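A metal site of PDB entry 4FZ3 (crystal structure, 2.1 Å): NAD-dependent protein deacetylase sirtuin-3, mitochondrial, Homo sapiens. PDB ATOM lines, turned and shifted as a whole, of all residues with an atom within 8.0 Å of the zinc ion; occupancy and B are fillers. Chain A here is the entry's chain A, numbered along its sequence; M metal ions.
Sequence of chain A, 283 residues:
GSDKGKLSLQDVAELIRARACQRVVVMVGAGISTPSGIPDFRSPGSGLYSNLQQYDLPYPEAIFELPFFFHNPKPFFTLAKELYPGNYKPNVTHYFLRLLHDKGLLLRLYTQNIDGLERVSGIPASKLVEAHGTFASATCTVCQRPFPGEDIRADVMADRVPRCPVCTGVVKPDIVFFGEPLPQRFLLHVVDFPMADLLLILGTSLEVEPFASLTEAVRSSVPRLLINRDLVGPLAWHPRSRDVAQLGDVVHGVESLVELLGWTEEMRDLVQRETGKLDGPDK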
ATOM      1  N   THR A 139     -16.090 -14.741 -11.212  1.00  0.00           N
ATOM      2  CA  THR A 139     -15.248 -15.713 -11.858  1.00  0.00           C
ATOM      3  C   THR A 139     -15.619 -17.162 -11.467  1.00  0.00           C
ATOM      4  O   THR A 139     -15.699 -17.456 -10.296  1.00  0.00           O
ATOM      5  CB  THR A 139     -13.745 -15.444 -11.507  1.00  0.00           C
ATOM      6  OG1 THR A 139     -13.346 -14.164 -12.065  1.00  0.00           O
ATOM      7  CG2 THR A 139     -12.841 -16.519 -12.082  1.00  0.00           C
ATOM      8  N   CYS A 140     -15.771 -18.030 -12.455  1.00  0.00           N
ATOM      9  CA  CYS A 140     -15.920 -19.443 -12.182  1.00  0.00           C
ATOM     10  C   CYS A 140     -14.765 -20.039 -11.333  1.00  0.00           C
ATOM     11  O   CYS A 140     -13.580 -20.038 -11.722  1.00  0.00           O
ATOM     12  CB  CYS A 140     -16.055 -20.256 -13.453  1.00  0.00           C
ATOM     13  SG  CYS A 140     -16.327 -22.063 -12.996  1.00  0.00           S
ATOM     14  N   THR A 141     -15.133 -20.598 -10.173  1.00  0.00           N
ATOM     15  CA  THR A 141     -14.092 -21.170  -9.288  1.00  0.00           C
ATOM     16  C   THR A 141     -13.474 -22.371  -9.912  1.00  0.00           C
ATOM     17  O   THR A 141     -12.454 -22.818  -9.422  1.00  0.00           O
ATOM     18  CB  THR A 141     -14.653 -21.597  -7.860  1.00  0.00           C
ATOM     19  OG1 THR A 141     -15.805 -22.428  -8.044  1.00  0.00           O
ATOM     20  CG2 THR A 141     -15.083 -20.329  -7.022  1.00  0.00           C
ATOM     21  N   VAL A 142     -14.046 -22.952 -10.952  1.00  0.00           N
ATOM     22  CA  VAL A 142     -13.457 -24.201 -11.451  1.00  0.00           C
ATOM     23  C   VAL A 142     -12.697 -23.981 -12.747  1.00  0.00           C
ATOM     24  O   VAL A 142     -11.532 -24.415 -12.873  1.00  0.00           O
ATOM     25  CB  VAL A 142     -14.480 -25.342 -11.563  1.00  0.00           C
ATOM     26  CG1 VAL A 142     -13.820 -26.567 -12.239  1.00  0.00           C
ATOM     27  CG2 VAL A 142     -15.032 -25.738 -10.150  1.00  0.00           C
ATOM     28  N   CYS A 143     -13.317 -23.358 -13.752  1.00  0.00           N
ATOM     29  CA  CYS A 143     -12.599 -23.248 -15.018  1.00  0.00           C
ATOM     30  C   CYS A 143     -12.000 -21.855 -15.226  1.00  0.00           C
ATOM     31  O   CYS A 143     -11.463 -21.580 -16.302  1.00  0.00           O
ATOM     32  CB  CYS A 143     -13.515 -23.567 -16.222  1.00  0.00           C
ATOM     33  SG  CYS A 143     -14.836 -22.290 -16.429  1.00  0.00           S
ATOM     34  N   GLN A 144     -12.155 -20.978 -14.249  1.00  0.00           N
ATOM     35  CA  GLN A 144     -11.660 -19.554 -14.322  1.00  0.00           C
ATOM     36  C   GLN A 144     -12.297 -18.650 -15.373  1.00  0.00           C
ATOM     37  O   GLN A 144     -11.792 -17.528 -15.622  1.00  0.00           O
ATOM     38  CB  GLN A 144     -10.138 -19.479 -14.455  1.00  0.00           C
ATOM     39  CG  GLN A 144      -9.368 -20.563 -13.669  1.00  0.00           C
ATOM     40  CD  GLN A 144      -9.859 -20.772 -12.218  1.00  0.00           C
ATOM     41  OE1 GLN A 144     -10.207 -19.810 -11.503  1.00  0.00           O
ATOM     42  NE2 GLN A 144      -9.862 -22.019 -11.779  1.00  0.00           N
ATOM     43  N   ARG A 145     -13.366 -19.090 -16.026  1.00  0.00           N
ATOM     44  CA  ARG A 145     -14.118 -18.141 -16.902  1.00  0.00           C
ATOM     45  C   ARG A 145     -14.620 -16.909 -16.180  1.00  0.00           C
ATOM     46  O   ARG A 145     -15.259 -17.008 -15.105  1.00  0.00           O
ATOM     47  CB  ARG A 145     -15.306 -18.812 -17.574  1.00  0.00           C
ATOM     48  CG  ARG A 145     -14.949 -19.618 -18.792  1.00  0.00           C
ATOM     49  CD  ARG A 145     -16.296 -20.175 -19.429  1.00  0.00           C
ATOM     50  NE  ARG A 145     -16.023 -20.847 -20.700  1.00  0.00           N
ATOM     51  CZ  ARG A 145     -15.568 -22.085 -20.873  1.00  0.00           C
ATOM     52  NH1 ARG A 145     -15.365 -22.514 -22.102  1.00  0.00           N
ATOM     53  NH2 ARG A 145     -15.314 -22.895 -19.842  1.00  0.00           N
ATOM     54  N   PRO A 146     -14.333 -15.699 -16.766  1.00  0.00           N
ATOM     55  CA  PRO A 146     -14.808 -14.415 -16.206  1.00  0.00           C
ATOM     56  C   PRO A 146     -16.266 -14.090 -16.547  1.00  0.00           C
ATOM     57  O   PRO A 146     -16.739 -14.489 -17.596  1.00  0.00           O
ATOM     58  CB  PRO A 146     -13.876 -13.380 -16.880  1.00  0.00           C
ATOM     59  CG  PRO A 146     -13.563 -14.032 -18.257  1.00  0.00           C
ATOM     60  CD  PRO A 146     -13.341 -15.524 -17.846  1.00  0.00           C
ATOM     61  N   PHE A 147     -16.996 -13.363 -15.701  1.00  0.00           N
ATOM     62  CA  PHE A 147     -18.386 -13.012 -16.039  1.00  0.00           C
ATOM     63  C   PHE A 147     -18.723 -11.676 -15.417  1.00  0.00           C
ATOM     64  O   PHE A 147     -18.345 -11.422 -14.288  1.00  0.00           O
ATOM     65  CB  PHE A 147     -19.459 -14.042 -15.537  1.00  0.00           C
ATOM     66  CG  PHE A 147     -19.308 -15.450 -16.064  1.00  0.00           C
ATOM     67  CD1 PHE A 147     -19.861 -15.828 -17.290  1.00  0.00           C
ATOM     68  CD2 PHE A 147     -18.623 -16.417 -15.289  1.00  0.00           C
ATOM     69  CE1 PHE A 147     -19.718 -17.142 -17.782  1.00  0.00           C
ATOM     70  CE2 PHE A 147     -18.487 -17.726 -15.770  1.00  0.00           C
ATOM     71  CZ  PHE A 147     -19.031 -18.073 -17.012  1.00  0.00           C
ATOM     72  N   ARG A 163     -24.093 -20.865 -10.952  1.00  0.00           N
ATOM     73  CA  ARG A 163     -23.268 -21.943 -11.512  1.00  0.00           C
ATOM     74  C   ARG A 163     -22.775 -21.671 -12.926  1.00  0.00           C
ATOM     75  O   ARG A 163     -23.435 -21.054 -13.726  1.00  0.00           O
ATOM     76  CB  ARG A 163     -23.993 -23.287 -11.443  1.00  0.00           C
ATOM     77  CG  ARG A 163     -24.181 -23.747 -10.016  1.00  0.00           C
ATOM     78  CD  ARG A 163     -24.188 -25.243  -9.808  1.00  0.00           C
ATOM     79  NE  ARG A 163     -23.897 -25.427  -8.419  1.00  0.00           N
ATOM     80  CZ  ARG A 163     -22.824 -25.950  -7.824  1.00  0.00           C
ATOM     81  NH1 ARG A 163     -21.833 -26.429  -8.557  1.00  0.00           N
ATOM     82  NH2 ARG A 163     -22.744 -25.985  -6.490  1.00  0.00           N
ATOM     83  N   CYS A 164     -21.560 -22.112 -13.195  1.00  0.00           N
ATOM     84  CA  CYS A 164     -20.927 -21.913 -14.513  1.00  0.00           C
ATOM     85  C   CYS A 164     -21.756 -22.541 -15.670  1.00  0.00           C
ATOM     86  O   CYS A 164     -22.071 -23.744 -15.624  1.00  0.00           O
ATOM     87  CB  CYS A 164     -19.521 -22.514 -14.498  1.00  0.00           C
ATOM     88  SG  CYS A 164     -18.639 -22.021 -16.035  1.00  0.00           S
ATOM     89  N   PRO A 165     -22.096 -21.757 -16.714  1.00  0.00           N
ATOM     90  CA  PRO A 165     -22.950 -22.316 -17.808  1.00  0.00           C
ATOM     91  C   PRO A 165     -22.193 -23.295 -18.702  1.00  0.00           C
ATOM     92  O   PRO A 165     -22.793 -23.936 -19.561  1.00  0.00           O
ATOM     93  CB  PRO A 165     -23.411 -21.058 -18.623  1.00  0.00           C
ATOM     94  CG  PRO A 165     -22.321 -20.023 -18.272  1.00  0.00           C
ATOM     95  CD  PRO A 165     -22.008 -20.301 -16.805  1.00  0.00           C
ATOM     96  N   VAL A 166     -20.898 -23.431 -18.456  1.00  0.00           N
ATOM     97  CA  VAL A 166     -20.129 -24.457 -19.175  1.00  0.00           C
ATOM     98  C   VAL A 166     -19.787 -25.645 -18.277  1.00  0.00           C
ATOM     99  O   VAL A 166     -20.130 -26.762 -18.614  1.00  0.00           O
ATOM    100  CB  VAL A 166     -18.786 -23.874 -19.804  1.00  0.00           C
ATOM    101  CG1 VAL A 166     -18.010 -24.966 -20.440  1.00  0.00           C
ATOM    102  CG2 VAL A 166     -19.091 -22.773 -20.845  1.00  0.00           C
ATOM    103  N   CYS A 167     -19.113 -25.413 -17.138  1.00  0.00           N
ATOM    104  CA  CYS A 167     -18.564 -26.552 -16.294  1.00  0.00           C
ATOM    105  C   CYS A 167     -19.362 -26.897 -15.014  1.00  0.00           C
ATOM    106  O   CYS A 167     -19.043 -27.856 -14.388  1.00  0.00           O
ATOM    107  CB  CYS A 167     -17.061 -26.340 -15.885  1.00  0.00           C
ATOM    108  SG  CYS A 167     -16.845 -25.244 -14.473  1.00  0.00           S
ATOM    109  N   THR A 168     -20.358 -26.096 -14.659  1.00  0.00           N
ATOM    110  CA  THR A 168     -21.208 -26.195 -13.465  1.00  0.00           C
ATOM    111  C   THR A 168     -20.562 -25.688 -12.177  1.00  0.00           C
ATOM    112  O   THR A 168     -21.217 -25.720 -11.114  1.00  0.00           O
ATOM    113  CB  THR A 168     -21.908 -27.618 -13.244  1.00  0.00           C
ATOM    114  OG1 THR A 168     -20.929 -28.485 -12.728  1.00  0.00           O
ATOM    115  CG2 THR A 168     -22.315 -28.237 -14.582  1.00  0.00           C
ATOM    116  N   GLY A 169     -19.323 -25.210 -12.241  1.00  0.00           N
ATOM    117  CA  GLY A 169     -18.578 -24.724 -11.059  1.00  0.00           C
ATOM    118  C   GLY A 169     -19.332 -23.552 -10.443  1.00  0.00           C
ATOM    119  O   GLY A 169     -20.012 -22.826 -11.169  1.00  0.00           O
ATOM    120  N   VAL A 170     -19.255 -23.372  -9.121  1.00  0.00           N
ATOM    121  CA  VAL A 170     -19.834 -22.175  -8.464  1.00  0.00           C
ATOM    122  C   VAL A 170     -19.160 -20.912  -9.036  1.00  0.00           C
ATOM    123  O   VAL A 170     -17.934 -20.878  -9.240  1.00  0.00           O
ATOM    124  CB  VAL A 170     -19.642 -22.245  -6.929  1.00  0.00           C
ATOM    125  CG1 VAL A 170     -20.036 -20.974  -6.210  1.00  0.00           C
ATOM    126  CG2 VAL A 170     -20.532 -23.407  -6.404  1.00  0.00           C
ATOM    127  N   VAL A 171     -19.953 -19.935  -9.392  1.00  0.00           N
ATOM    128  CA  VAL A 171     -19.363 -18.700  -9.862  1.00  0.00           C
ATOM    129  C   VAL A 171     -19.248 -17.723  -8.731  1.00  0.00           C
ATOM    130  O   VAL A 171     -20.267 -17.357  -8.168  1.00  0.00           O
ATOM    131  CB  VAL A 171     -20.195 -18.134 -11.039  1.00  0.00           C
ATOM    132  CG1 VAL A 171     -19.659 -16.783 -11.475  1.00  0.00           C
ATOM    133  CG2 VAL A 171     -20.117 -19.142 -12.200  1.00  0.00           C
HETATM  134 ZN    ZN M   1     -16.707 -22.920 -15.186  1.00  0.00          ZN
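The nearest printed residue that does not touch the zinc ion is Gly 169 (4.6 Å).
The backbone NH (N) of Cys 164 sits at hydrogen-bond distance from the backbone carbonyl oxygen (O) of Gly 169 (2.6 Å).
The side-chain sulfur (SG) of Cys 164 lies close to the backbone NH (N) of Val 166, 3.6 Å away.
NH2 of Arg 145 sits close to SG of Cys 143, 3.5 Å away.
The side-chain sulfur (SG) of Cys 140 lies close to the backbone NH (N) of Val 142, 3.2 Å away.
The backbone NH (N) of Cys 140 sits at hydrogen-bond distance from the backbone carbonyl oxygen (O) of Arg 145 (2.9 Å).
The side-chain amide oxygen of Gln 144 sits close to the backbone carbonyl oxygen of Cys 140 (3.4 Å).
The side-chain sulfur (SG) of Cys 167 sits close to the backbone NH (N) of Gly 169 (3.3 Å).
The zinc ion is bound by the side-chain sulfur of Cys 164 (2.3 Å), the side-chain sulfur of Cys 143 (2.3 Å), the side-chain sulfur of Cys 140 (2.4 Å) and the side-chain sulfur of Cys 167 (2.4 Å).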
